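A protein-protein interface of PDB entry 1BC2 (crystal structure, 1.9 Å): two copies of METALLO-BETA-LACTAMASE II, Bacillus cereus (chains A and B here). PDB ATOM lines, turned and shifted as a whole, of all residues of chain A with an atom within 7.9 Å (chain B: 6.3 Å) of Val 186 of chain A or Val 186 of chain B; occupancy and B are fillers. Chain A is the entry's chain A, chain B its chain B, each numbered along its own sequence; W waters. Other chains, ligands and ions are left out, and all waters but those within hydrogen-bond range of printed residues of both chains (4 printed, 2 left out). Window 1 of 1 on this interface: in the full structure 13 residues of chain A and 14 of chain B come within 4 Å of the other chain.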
ATOM      1  N   LYS A 147     -33.788  15.296  12.639  1.00  0.00           N
ATOM      2  CA  LYS A 147     -32.557  15.129  13.410  1.00  0.00           C
ATOM      3  C   LYS A 147     -32.282  16.218  14.455  1.00  0.00           C
ATOM      4  O   LYS A 147     -32.489  17.401  14.208  1.00  0.00           O
ATOM      5  CB  LYS A 147     -31.375  15.015  12.449  1.00  0.00           C
ATOM      6  CG  LYS A 147     -31.562  13.944  11.388  1.00  0.00           C
ATOM      7  CD  LYS A 147     -30.469  14.023  10.369  1.00  0.00           C
ATOM      8  CE  LYS A 147     -30.722  13.072   9.235  1.00  0.00           C
ATOM      9  NZ  LYS A 147     -29.660  13.248   8.212  1.00  0.00           N
ATOM     10  N   GLY A 148     -31.791  15.802  15.617  1.00  0.00           N
ATOM     11  CA  GLY A 148     -31.485  16.738  16.690  1.00  0.00           C
ATOM     12  C   GLY A 148     -30.460  16.118  17.621  1.00  0.00           C
ATOM     13  O   GLY A 148     -29.291  15.998  17.248  1.00  0.00           O
ATOM     14  N   HIS A 149     -30.897  15.721  18.820  1.00  0.00           N
ATOM     15  CA  HIS A 149     -30.030  15.067  19.809  1.00  0.00           C
ATOM     16  C   HIS A 149     -29.334  13.867  19.157  1.00  0.00           C
ATOM     17  O   HIS A 149     -28.173  13.558  19.452  1.00  0.00           O
ATOM     18  CB  HIS A 149     -30.856  14.597  21.010  1.00  0.00           C
ATOM     19  CG  HIS A 149     -30.123  13.650  21.916  1.00  0.00           C
ATOM     20  ND1 HIS A 149     -28.958  14.001  22.573  1.00  0.00           N
ATOM     21  CD2 HIS A 149     -30.367  12.365  22.236  1.00  0.00           C
ATOM     22  CE1 HIS A 149     -28.520  12.960  23.255  1.00  0.00           C
ATOM     23  NE2 HIS A 149     -29.350  11.955  23.074  1.00  0.00           N
ATOM     24  N   THR A 150     -30.090  13.170  18.313  1.00  0.00           N
ATOM     25  CA  THR A 150     -29.612  12.031  17.551  1.00  0.00           C
ATOM     26  C   THR A 150     -30.290  12.104  16.195  1.00  0.00           C
ATOM     27  O   THR A 150     -31.155  12.956  15.956  1.00  0.00           O
ATOM     28  CB  THR A 150     -29.951  10.672  18.209  1.00  0.00           C
ATOM     29  OG1 THR A 150     -31.347  10.608  18.522  1.00  0.00           O
ATOM     30  CG2 THR A 150     -29.142  10.462  19.468  1.00  0.00           C
ATOM     31  N   LEU A 178     -25.897  20.798  26.306  1.00  0.00           N
ATOM     32  CA  LEU A 178     -26.719  19.987  25.413  1.00  0.00           C
ATOM     33  C   LEU A 178     -26.475  18.496  25.588  1.00  0.00           C
ATOM     34  O   LEU A 178     -27.224  17.683  25.050  1.00  0.00           O
ATOM     35  CB  LEU A 178     -26.432  20.341  23.962  1.00  0.00           C
ATOM     36  CG  LEU A 178     -26.822  21.746  23.532  1.00  0.00           C
ATOM     37  CD1 LEU A 178     -26.302  22.006  22.125  1.00  0.00           C
ATOM     38  CD2 LEU A 178     -28.329  21.899  23.614  1.00  0.00           C
ATOM     39  N   GLY A 179     -25.421  18.139  26.318  1.00  0.00           N
ATOM     40  CA  GLY A 179     -25.095  16.737  26.513  1.00  0.00           C
ATOM     41  C   GLY A 179     -24.262  16.210  25.356  1.00  0.00           C
ATOM     42  O   GLY A 179     -23.562  16.985  24.694  1.00  0.00           O
ATOM     43  N   ASN A 180     -24.337  14.899  25.113  1.00  0.00           N
ATOM     44  CA  ASN A 180     -23.593  14.242  24.031  1.00  0.00           C
ATOM     45  C   ASN A 180     -24.025  14.776  22.677  1.00  0.00           C
ATOM     46  O   ASN A 180     -25.156  14.556  22.242  1.00  0.00           O
ATOM     47  CB  ASN A 180     -23.801  12.713  24.079  1.00  0.00           C
ATOM     48  CG  ASN A 180     -23.143  11.968  22.900  1.00  0.00           C
ATOM     49  OD1 ASN A 180     -22.668  12.569  21.939  1.00  0.00           O
ATOM     50  ND2 ASN A 180     -23.127  10.645  22.984  1.00  0.00           N
ATOM     51  N   VAL A 181     -23.095  15.457  22.012  1.00  0.00           N
ATOM     52  CA  VAL A 181     -23.344  16.019  20.698  1.00  0.00           C
ATOM     53  C   VAL A 181     -22.523  15.301  19.637  1.00  0.00           C
ATOM     54  O   VAL A 181     -22.493  15.720  18.484  1.00  0.00           O
ATOM     55  CB  VAL A 181     -23.053  17.527  20.663  1.00  0.00           C
ATOM     56  CG1 VAL A 181     -24.018  18.264  21.585  1.00  0.00           C
ATOM     57  CG2 VAL A 181     -21.607  17.799  21.067  1.00  0.00           C
ATOM     58  N   ALA A 182     -21.854  14.219  20.026  1.00  0.00           N
ATOM     59  CA  ALA A 182     -21.065  13.445  19.075  1.00  0.00           C
ATOM     60  C   ALA A 182     -22.009  12.762  18.084  1.00  0.00           C
ATOM     61  O   ALA A 182     -21.700  12.666  16.898  1.00  0.00           O
ATOM     62  CB  ALA A 182     -20.218  12.416  19.798  1.00  0.00           C
ATOM     63  N   ASP A 183     -23.177  12.333  18.568  1.00  0.00           N
ATOM     64  CA  ASP A 183     -24.183  11.663  17.730  1.00  0.00           C
ATOM     65  C   ASP A 183     -25.268  12.636  17.253  1.00  0.00           C
ATOM     66  O   ASP A 183     -26.150  12.276  16.469  1.00  0.00           O
ATOM     67  CB  ASP A 183     -24.852  10.525  18.507  1.00  0.00           C
ATOM     68  CG  ASP A 183     -23.855   9.537  19.081  1.00  0.00           C
ATOM     69  OD1 ASP A 183     -22.943   9.113  18.349  1.00  0.00           O
ATOM     70  OD2 ASP A 183     -23.981   9.180  20.271  1.00  0.00           O
ATOM     71  N   ALA A 184     -25.181  13.875  17.716  1.00  0.00           N
ATOM     72  CA  ALA A 184     -26.154  14.895  17.381  1.00  0.00           C
ATOM     73  C   ALA A 184     -25.945  15.614  16.061  1.00  0.00           C
ATOM     74  O   ALA A 184     -24.892  15.519  15.428  1.00  0.00           O
ATOM     75  CB  ALA A 184     -26.236  15.904  18.505  1.00  0.00           C
ATOM     76  N   TYR A 185     -27.008  16.296  15.641  1.00  0.00           N
ATOM     77  CA  TYR A 185     -27.031  17.110  14.434  1.00  0.00           C
ATOM     78  C   TYR A 185     -27.456  18.485  14.948  1.00  0.00           C
ATOM     79  O   TYR A 185     -28.636  18.866  14.888  1.00  0.00           O
ATOM     80  CB  TYR A 185     -28.036  16.551  13.435  1.00  0.00           C
ATOM     81  CG  TYR A 185     -27.639  15.198  12.915  1.00  0.00           C
ATOM     82  CD1 TYR A 185     -27.771  14.061  13.709  1.00  0.00           C
ATOM     83  CD2 TYR A 185     -27.094  15.058  11.641  1.00  0.00           C
ATOM     84  CE1 TYR A 185     -27.362  12.820  13.252  1.00  0.00           C
ATOM     85  CE2 TYR A 185     -26.684  13.819  11.170  1.00  0.00           C
ATOM     86  CZ  TYR A 185     -26.817  12.701  11.980  1.00  0.00           C
ATOM     87  OH  TYR A 185     -26.392  11.467  11.520  1.00  0.00           O
ATOM     88  N   VAL A 186     -26.467  19.189  15.500  1.00  0.00           N
ATOM     89  CA  VAL A 186     -26.633  20.499  16.118  1.00  0.00           C
ATOM     90  C   VAL A 186     -27.355  21.542  15.287  1.00  0.00           C
ATOM     91  O   VAL A 186     -28.254  22.210  15.790  1.00  0.00           O
ATOM     92  CB  VAL A 186     -25.272  21.059  16.604  1.00  0.00           C
ATOM     93  CG1 VAL A 186     -25.453  22.432  17.241  1.00  0.00           C
ATOM     94  CG2 VAL A 186     -24.659  20.109  17.609  1.00  0.00           C
ATOM     95  N   ASN A 187     -26.973  21.672  14.022  1.00  0.00           N
ATOM     96  CA  ASN A 187     -27.590  22.651  13.136  1.00  0.00           C
ATOM     97  C   ASN A 187     -29.072  22.384  12.869  1.00  0.00           C
ATOM     98  O   ASN A 187     -29.887  23.308  12.882  1.00  0.00           O
ATOM     99  CB  ASN A 187     -26.830  22.724  11.811  1.00  0.00           C
ATOM    100  CG  ASN A 187     -27.309  23.861  10.928  1.00  0.00           C
ATOM    101  OD1 ASN A 187     -27.139  25.033  11.268  1.00  0.00           O
ATOM    102  ND2 ASN A 187     -27.910  23.523   9.787  1.00  0.00           N
ATOM    103  N   GLU A 188     -29.419  21.120  12.647  1.00  0.00           N
ATOM    104  CA  GLU A 188     -30.801  20.736  12.363  1.00  0.00           C
ATOM    105  C   GLU A 188     -31.701  20.624  13.581  1.00  0.00           C
ATOM    106  O   GLU A 188     -32.924  20.717  13.461  1.00  0.00           O
ATOM    107  CB  GLU A 188     -30.831  19.426  11.553  1.00  0.00           C
ATOM    108  CG  GLU A 188     -30.608  19.596  10.021  1.00  0.00           C
ATOM    109  CD  GLU A 188     -31.695  20.524   9.447  1.00  0.00           C
ATOM    110  OE1 GLU A 188     -32.903  20.263   9.740  1.00  0.00           O
ATOM    111  OE2 GLU A 188     -31.355  21.467   8.685  1.00  0.00           O
ATOM    112  N   TRP A 189     -31.079  20.433  14.742  1.00  0.00           N
ATOM    113  CA  TRP A 189     -31.780  20.317  16.011  1.00  0.00           C
ATOM    114  C   TRP A 189     -32.772  21.488  16.160  1.00  0.00           C
ATOM    115  O   TRP A 189     -33.919  21.289  16.575  1.00  0.00           O
ATOM    116  CB  TRP A 189     -30.742  20.299  17.140  1.00  0.00           C
ATOM    117  CG  TRP A 189     -31.225  19.838  18.473  1.00  0.00           C
ATOM    118  CD1 TRP A 189     -32.492  19.910  18.960  1.00  0.00           C
ATOM    119  CD2 TRP A 189     -30.420  19.310  19.528  1.00  0.00           C
ATOM    120  NE1 TRP A 189     -32.526  19.477  20.259  1.00  0.00           N
ATOM    121  CE2 TRP A 189     -31.264  19.100  20.633  1.00  0.00           C
ATOM    122  CE3 TRP A 189     -29.057  19.002  19.649  1.00  0.00           C
ATOM    123  CZ2 TRP A 189     -30.797  18.595  21.849  1.00  0.00           C
ATOM    124  CZ3 TRP A 189     -28.591  18.497  20.865  1.00  0.00           C
ATOM    125  CH2 TRP A 189     -29.460  18.301  21.944  1.00  0.00           C
ATOM    126  N   SER A 190     -32.366  22.686  15.738  1.00  0.00           N
ATOM    127  CA  SER A 190     -33.234  23.863  15.816  1.00  0.00           C
ATOM    128  C   SER A 190     -34.477  23.746  14.926  1.00  0.00           C
ATOM    129  O   SER A 190     -35.592  24.056  15.364  1.00  0.00           O
ATOM    130  CB  SER A 190     -32.452  25.129  15.482  1.00  0.00           C
ATOM    131  OG  SER A 190     -31.609  25.480  16.566  1.00  0.00           O
ATOM    132  N   THR A 191     -34.286  23.305  13.684  1.00  0.00           N
ATOM    133  CA  THR A 191     -35.404  23.130  12.761  1.00  0.00           C
ATOM    134  C   THR A 191     -36.357  22.045  13.276  1.00  0.00           C
ATOM    135  O   THR A 191     -37.570  22.150  13.111  1.00  0.00           O
ATOM    136  CB  THR A 191     -34.910  22.741  11.353  1.00  0.00           C
ATOM    137  OG1 THR A 191     -34.060  23.776  10.849  1.00  0.00           O
ATOM    138  CG2 THR A 191     -36.086  22.561  10.399  1.00  0.00           C
ATOM    139  N   SER A 192     -35.808  21.026  13.934  1.00  0.00           N
ATOM    140  CA  SER A 192     -36.618  19.934  14.458  1.00  0.00           C
ATOM    141  C   SER A 192     -37.483  20.342  15.636  1.00  0.00           C
ATOM    142  O   SER A 192     -38.599  19.848  15.786  1.00  0.00           O
ATOM    143  CB  SER A 192     -35.746  18.743  14.808  1.00  0.00           C
ATOM    144  OG  SER A 192     -35.070  18.309  13.650  1.00  0.00           O
ATOM    145  N   LEU A 223     -33.767  25.974  22.305  1.00  0.00           N
ATOM    146  CA  LEU A 223     -33.454  26.712  21.078  1.00  0.00           C
ATOM    147  C   LEU A 223     -32.435  27.802  21.424  1.00  0.00           C
ATOM    148  O   LEU A 223     -31.544  28.123  20.635  1.00  0.00           O
ATOM    149  CB  LEU A 223     -34.720  27.352  20.478  1.00  0.00           C
ATOM    150  CG  LEU A 223     -35.716  26.509  19.657  1.00  0.00           C
ATOM    151  CD1 LEU A 223     -37.000  27.299  19.408  1.00  0.00           C
ATOM    152  CD2 LEU A 223     -35.096  26.072  18.340  1.00  0.00           C
ATOM    153  N   ASP A 224     -32.557  28.339  22.633  1.00  0.00           N
ATOM    154  CA  ASP A 224     -31.653  29.377  23.092  1.00  0.00           C
ATOM    155  C   ASP A 224     -30.251  28.799  23.180  1.00  0.00           C
ATOM    156  O   ASP A 224     -29.309  29.383  22.655  1.00  0.00           O
ATOM    157  CB  ASP A 224     -32.105  29.913  24.451  1.00  0.00           C
ATOM    158  CG  ASP A 224     -31.267  31.091  24.928  1.00  0.00           C
ATOM    159  OD1 ASP A 224     -30.697  31.815  24.080  1.00  0.00           O
ATOM    160  OD2 ASP A 224     -31.179  31.298  26.155  1.00  0.00           O
ATOM    161  N   LEU A 225     -30.130  27.633  23.814  1.00  0.00           N
ATOM    162  CA  LEU A 225     -28.850  26.947  23.966  1.00  0.00           C
ATOM    163  C   LEU A 225     -28.205  26.606  22.621  1.00  0.00           C
ATOM    164  O   LEU A 225     -26.973  26.596  22.499  1.00  0.00           O
ATOM    165  CB  LEU A 225     -29.022  25.653  24.764  1.00  0.00           C
ATOM    166  CG  LEU A 225     -29.456  25.700  26.227  1.00  0.00           C
ATOM    167  CD1 LEU A 225     -29.434  24.272  26.770  1.00  0.00           C
ATOM    168  CD2 LEU A 225     -28.537  26.601  27.040  1.00  0.00           C
ATOM    169  N   LEU A 226     -29.041  26.324  21.622  1.00  0.00           N
ATOM    170  CA  LEU A 226     -28.580  25.968  20.282  1.00  0.00           C
ATOM    171  C   LEU A 226     -28.113  27.148  19.439  1.00  0.00           C
ATOM    172  O   LEU A 226     -27.409  26.952  18.449  1.00  0.00           O
ATOM    173  CB  LEU A 226     -29.679  25.217  19.529  1.00  0.00           C
ATOM    174  CG  LEU A 226     -29.915  23.798  20.034  1.00  0.00           C
ATOM    175  CD1 LEU A 226     -31.277  23.300  19.613  1.00  0.00           C
ATOM    176  CD2 LEU A 226     -28.798  22.900  19.517  1.00  0.00           C
ATOM    177  N   LYS A 227     -28.500  28.361  19.818  1.00  0.00           N
ATOM    178  CA  LYS A 227     -28.109  29.547  19.058  1.00  0.00           C
ATOM    179  C   LYS A 227     -26.599  29.731  18.912  1.00  0.00           C
ATOM    180  O   LYS A 227     -26.148  29.901  17.766  1.00  0.00           O
ATOM    181  CB  LYS A 227     -28.740  30.806  19.654  1.00  0.00           C
ATOM    182  CG  LYS A 227     -30.241  30.875  19.473  1.00  0.00           C
ATOM    183  CD  LYS A 227     -30.776  32.257  19.803  1.00  0.00           C
ATOM    184  CE  LYS A 227     -32.250  32.373  19.428  1.00  0.00           C
ATOM    185  NZ  LYS A 227     -32.803  33.750  19.632  1.00  0.00           N
ATOM    186  OXT LYS A 227     -25.882  29.693  19.930  1.00  0.00           O
ATOM    187  N   GLY B 148     -17.682  32.114  19.923  1.00  0.00           N
ATOM    188  CA  GLY B 148     -17.686  30.664  19.934  1.00  0.00           C
ATOM    189  C   GLY B 148     -18.236  30.218  21.272  1.00  0.00           C
ATOM    190  O   GLY B 148     -19.430  30.371  21.536  1.00  0.00           O
ATOM    191  N   LEU B 178     -19.778  19.626  24.352  1.00  0.00           N
ATOM    192  CA  LEU B 178     -19.294  20.964  24.030  1.00  0.00           C
ATOM    193  C   LEU B 178     -19.193  21.820  25.292  1.00  0.00           C
ATOM    194  O   LEU B 178     -18.561  22.877  25.284  1.00  0.00           O
ATOM    195  CB  LEU B 178     -20.215  21.654  23.019  1.00  0.00           C
ATOM    196  CG  LEU B 178     -20.139  21.267  21.540  1.00  0.00           C
ATOM    197  CD1 LEU B 178     -21.248  21.969  20.780  1.00  0.00           C
ATOM    198  CD2 LEU B 178     -18.791  21.649  20.967  1.00  0.00           C
ATOM    199  N   VAL B 181     -23.161  26.038  26.982  1.00  0.00           N
ATOM    200  CA  VAL B 181     -23.462  26.825  25.789  1.00  0.00           C
ATOM    201  C   VAL B 181     -24.480  27.934  26.014  1.00  0.00           C
ATOM    202  O   VAL B 181     -24.905  28.589  25.063  1.00  0.00           O
ATOM    203  CB  VAL B 181     -23.937  25.938  24.616  1.00  0.00           C
ATOM    204  CG1 VAL B 181     -22.785  25.066  24.117  1.00  0.00           C
ATOM    205  CG2 VAL B 181     -25.130  25.087  25.044  1.00  0.00           C
ATOM    206  N   ALA B 184     -22.871  30.707  24.799  1.00  0.00           N
ATOM    207  CA  ALA B 184     -22.196  30.419  23.542  1.00  0.00           C
ATOM    208  C   ALA B 184     -22.962  30.883  22.318  1.00  0.00           C
ATOM    209  O   ALA B 184     -24.141  31.240  22.391  1.00  0.00           O
ATOM    210  CB  ALA B 184     -21.897  28.930  23.433  1.00  0.00           C
ATOM    211  N   TYR B 185     -22.246  30.930  21.202  1.00  0.00           N
ATOM    212  CA  TYR B 185     -22.800  31.304  19.908  1.00  0.00           C
ATOM    213  C   TYR B 185     -22.413  30.112  19.049  1.00  0.00           C
ATOM    214  O   TYR B 185     -21.428  30.136  18.306  1.00  0.00           O
ATOM    215  CB  TYR B 185     -22.166  32.602  19.400  1.00  0.00           C
ATOM    216  CG  TYR B 185     -22.530  33.815  20.232  1.00  0.00           C
ATOM    217  CD1 TYR B 185     -21.892  34.065  21.448  1.00  0.00           C
ATOM    218  CD2 TYR B 185     -23.522  34.700  19.813  1.00  0.00           C
ATOM    219  CE1 TYR B 185     -22.235  35.161  22.228  1.00  0.00           C
ATOM    220  CE2 TYR B 185     -23.870  35.803  20.586  1.00  0.00           C
ATOM    221  CZ  TYR B 185     -23.222  36.027  21.792  1.00  0.00           C
ATOM    222  OH  TYR B 185     -23.557  37.118  22.561  1.00  0.00           O
ATOM    223  N   VAL B 186     -23.167  29.038  19.247  1.00  0.00           N
ATOM    224  CA  VAL B 186     -22.961  27.766  18.576  1.00  0.00           C
ATOM    225  C   VAL B 186     -22.800  27.839  17.064  1.00  0.00           C
ATOM    226  O   VAL B 186     -21.932  27.167  16.505  1.00  0.00           O
ATOM    227  CB  VAL B 186     -24.079  26.771  18.964  1.00  0.00           C
ATOM    228  CG1 VAL B 186     -23.858  25.420  18.310  1.00  0.00           C
ATOM    229  CG2 VAL B 186     -24.114  26.625  20.475  1.00  0.00           C
ATOM    230  N   ASN B 187     -23.607  28.662  16.404  1.00  0.00           N
ATOM    231  CA  ASN B 187     -23.509  28.778  14.956  1.00  0.00           C
ATOM    232  C   ASN B 187     -22.283  29.552  14.491  1.00  0.00           C
ATOM    233  O   ASN B 187     -21.741  29.267  13.427  1.00  0.00           O
ATOM    234  CB  ASN B 187     -24.769  29.397  14.361  1.00  0.00           C
ATOM    235  CG  ASN B 187     -24.777  29.341  12.842  1.00  0.00           C
ATOM    236  OD1 ASN B 187     -24.678  28.263  12.242  1.00  0.00           O
ATOM    237  ND2 ASN B 187     -24.867  30.506  12.211  1.00  0.00           N
ATOM    238  N   GLU B 188     -21.841  30.521  15.285  1.00  0.00           N
ATOM    239  CA  GLU B 188     -20.673  31.319  14.925  1.00  0.00           C
ATOM    240  C   GLU B 188     -19.356  30.614  15.274  1.00  0.00           C
ATOM    241  O   GLU B 188     -18.313  30.873  14.661  1.00  0.00           O
ATOM    242  CB  GLU B 188     -20.749  32.695  15.588  1.00  0.00           C
ATOM    243  CG  GLU B 188     -21.948  33.513  15.122  1.00  0.00           C
ATOM    244  CD  GLU B 188     -21.898  34.960  15.578  1.00  0.00           C
ATOM    245  OE1 GLU B 188     -20.814  35.574  15.488  1.00  0.00           O
ATOM    246  OE2 GLU B 188     -22.944  35.489  16.014  1.00  0.00           O
ATOM    247  N   TRP B 189     -19.435  29.684  16.225  1.00  0.00           N
ATOM    248  CA  TRP B 189     -18.295  28.903  16.700  1.00  0.00           C
ATOM    249  C   TRP B 189     -17.494  28.273  15.553  1.00  0.00           C
ATOM    250  O   TRP B 189     -16.266  28.414  15.496  1.00  0.00           O
ATOM    251  CB  TRP B 189     -18.804  27.819  17.654  1.00  0.00           C
ATOM    252  CG  TRP B 189     -17.786  27.213  18.594  1.00  0.00           C
ATOM    253  CD1 TRP B 189     -16.445  27.027  18.366  1.00  0.00           C
ATOM    254  CD2 TRP B 189     -18.052  26.650  19.883  1.00  0.00           C
ATOM    255  NE1 TRP B 189     -15.871  26.379  19.431  1.00  0.00           N
ATOM    256  CE2 TRP B 189     -16.833  26.138  20.380  1.00  0.00           C
ATOM    257  CE3 TRP B 189     -19.211  26.526  20.672  1.00  0.00           C
ATOM    258  CZ2 TRP B 189     -16.735  25.501  21.630  1.00  0.00           C
ATOM    259  CZ3 TRP B 189     -19.114  25.890  21.916  1.00  0.00           C
ATOM    260  CH2 TRP B 189     -17.881  25.391  22.382  1.00  0.00           C
ATOM    261  N   SER B 190     -18.183  27.600  14.634  1.00  0.00           N
ATOM    262  CA  SER B 190     -17.508  26.959  13.510  1.00  0.00           C
ATOM    263  C   SER B 190     -16.656  27.918  12.694  1.00  0.00           C
ATOM    264  O   SER B 190     -15.511  27.606  12.367  1.00  0.00           O
ATOM    265  CB  SER B 190     -18.507  26.246  12.597  1.00  0.00           C
ATOM    266  OG  SER B 190     -18.912  25.011  13.157  1.00  0.00           O
ATOM    267  N   LEU B 225     -18.035  18.058  16.294  1.00  0.00           N
ATOM    268  CA  LEU B 225     -18.988  18.155  17.396  1.00  0.00           C
ATOM    269  C   LEU B 225     -20.022  19.245  17.123  1.00  0.00           C
ATOM    270  O   LEU B 225     -21.188  19.111  17.487  1.00  0.00           O
ATOM    271  CB  LEU B 225     -18.280  18.459  18.732  1.00  0.00           C
ATOM    272  CG  LEU B 225     -17.358  17.420  19.384  1.00  0.00           C
ATOM    273  CD1 LEU B 225     -16.898  17.905  20.746  1.00  0.00           C
ATOM    274  CD2 LEU B 225     -18.081  16.092  19.533  1.00  0.00           C
ATOM    275  N   LEU B 226     -19.596  20.311  16.454  1.00  0.00           N
ATOM    276  CA  LEU B 226     -20.486  21.427  16.145  1.00  0.00           C
ATOM    277  C   LEU B 226     -21.468  21.211  15.000  1.00  0.00           C
ATOM    278  O   LEU B 226     -22.459  21.925  14.903  1.00  0.00           O
ATOM    279  CB  LEU B 226     -19.674  22.695  15.882  1.00  0.00           C
ATOM    280  CG  LEU B 226     -19.028  23.321  17.120  1.00  0.00           C
ATOM    281  CD1 LEU B 226     -17.918  24.265  16.705  1.00  0.00           C
ATOM    282  CD2 LEU B 226     -20.088  24.027  17.963  1.00  0.00           C
ATOM    283  N   LYS B 227     -21.203  20.232  14.139  1.00  0.00           N
ATOM    284  CA  LYS B 227     -22.079  19.968  12.998  1.00  0.00           C
ATOM    285  C   LYS B 227     -23.512  19.629  13.382  1.00  0.00           C
ATOM    286  O   LYS B 227     -24.426  20.187  12.743  1.00  0.00           O
ATOM    287  CB  LYS B 227     -21.498  18.864  12.111  1.00  0.00           C
ATOM    288  CG  LYS B 227     -20.230  19.272  11.387  1.00  0.00           C
ATOM    289  CD  LYS B 227     -19.694  18.161  10.511  1.00  0.00           C
ATOM    290  CE  LYS B 227     -18.375  18.565   9.879  1.00  0.00           C
ATOM    291  NZ  LYS B 227     -17.827  17.479   9.031  1.00  0.00           N
ATOM    292  OXT LYS B 227     -23.699  18.813  14.307  1.00  0.00           O
HETATM  293  O   HOH W   1     -22.564  19.469  24.402  1.00  0.00           O
HETATM  294  O   HOH W   2     -24.111  31.674  16.837  1.00  0.00           O
HETATM  295  O   HOH W   3     -25.509  25.701  13.907  1.00  0.00           O
HETATM  296  O   HOH W   4     -27.032  19.217  11.797  1.00  0.00           O
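The backbone NH (N) of Asn 187 of chain B lies within hydrogen-bond range of the chain-end carboxylate (O) of Lys 227 of chain A, 3.1 Å away.
The backbone carbonyl oxygen (O) of Ala 184 of chain B sits close to the chain-end carboxylate (OXT) of Lys 227 of chain A.
N of Val 186 of chain A is in hydrogen-bond range of OXT of Lys 227 of chain B (3.0 Å).
The backbone NH of Val 186 of chain B is in hydrogen-bond range of the chain-end carboxylate of Lys 227 of chain A (2.9 Å).
The backbone NH (N) of Asn 187 of chain A is in hydrogen-bond range of the chain-end carboxylate (O) of Lys 227 of chain B (3.2 Å).
N of Tyr 185 of chain A is in hydrogen-bond range of O of Gly 148 of chain A (2.8 Å).
N of Ala 184 of chain A lies close to O of His 149 of chain A.
The backbone carbonyl oxygen (O) of Gly 148 of chain B is in hydrogen-bond range of the backbone NH (N) of Tyr 185 of chain B (2.9 Å).
Among the printed residues, pairs that only touch across the chains: Val 181 of chain A with Leu 178 of chain B (3.8 Å), Val 181 of chain A with Leu 225 of chain B (3.8 Å), Ala 184 of chain A with Lys 227 of chain B (3.7 Å), Tyr 185 of chain A with Lys 227 of chain B (3.7 Å), Val 186 of chain A with Val 186 of chain B (3.6 Å), Val 186 of chain A with Leu 225 of chain B (3.6 Å), Val 186 of chain A with Leu 226 of chain B (3.4 Å), Leu 225 of chain A with Val 181 of chain B (3.5 Å), Leu 225 of chain A with Val 186 of chain B (3.5 Å), Leu 226 of chain A with Val 186 of chain B (3.4 Å) and Lys 227 of chain A with Tyr 185 of chain B (3.5 Å).
Gly 148 of chain A touches none of the printed residues of chain B.
Of the printed residues of chain A, Tyr 185 of chain B touches Lys 227 (3.5 Å).
Of the printed residues of chain A, Val 186 of chain B touches Val 186, Leu 225, Leu 226 and Lys 227.
Printed residues of chain A within 4 Å of Asn 187 of chain B: Lys 227 (3.1 Å).
The nearest residue of chain B that does not touch Val 186 of chain A is Leu 178 of chain B (5.0 Å).
The nearest printed residue of chain A that does not touch Leu 225 of chain B is Ala 182 of chain A (4.02 Å).
Of the 13 printed residues of chain B, 9 touch a printed residue of chain A.
Hydrophobic or aromatic side chains of chain B within 4 Å of the printed part of chain A: Leu 178, Val 181 and Val 186.
Along chain A the printed residues that touch a printed residue of chain B span positions 181 to 227.
Among the printed residues, 16 pairs touch across the chains.
Val 181 of chain A touches Leu 178 of chain B, but with the chains exchanged Leu 178 of chain A does not touch Val 181 of chain B (4.04 Å).
Tyr 185 of chain A touches Lys 227 of chain B, and with the chains exchanged Lys 227 of chain A touches Tyr 185 of chain B.
Val 186 of chain A touches Leu 226 of chain B, and with the chains exchanged Leu 226 of chain A touches Val 186 of chain B.
Val 186 of chain A touches Lys 227 of chain B, and with the chains exchanged Lys 227 of chain A touches Val 186 of chain B.
Positions printed for both chains: 148, 178, 181, 184, 185, 186, 187, 188, 189, 190, 225, 226 and 227.
Water W1 bridges the backbone carbonyl oxygen (O) of Gly 179 of chain A (2.7 Å) and the backbone NH (N) of Leu 178 of chain B (2.8 Å).
Water W2 lies within hydrogen-bond range of O of Lys 227 of chain A (2.9 Å), N of Glu 188 of chain B (3.0 Å), N of Asn 187 of chain B (3.1 Å) and O of Tyr 185 of chain B (3.4 Å).
Water W4 lies within hydrogen-bond range of the chain-end carboxylate (O) of Lys 227 of chain B (2.9 Å), the backbone NH (N) of Glu 188 of chain A (3.2 Å) and the backbone NH (N) of Asn 187 of chain A (3.3 Å).
Water W3 bridges OD1 of Asn 187 of chain B (3.2 Å) and OD1 of Asn 187 of chain A (3.2 Å).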
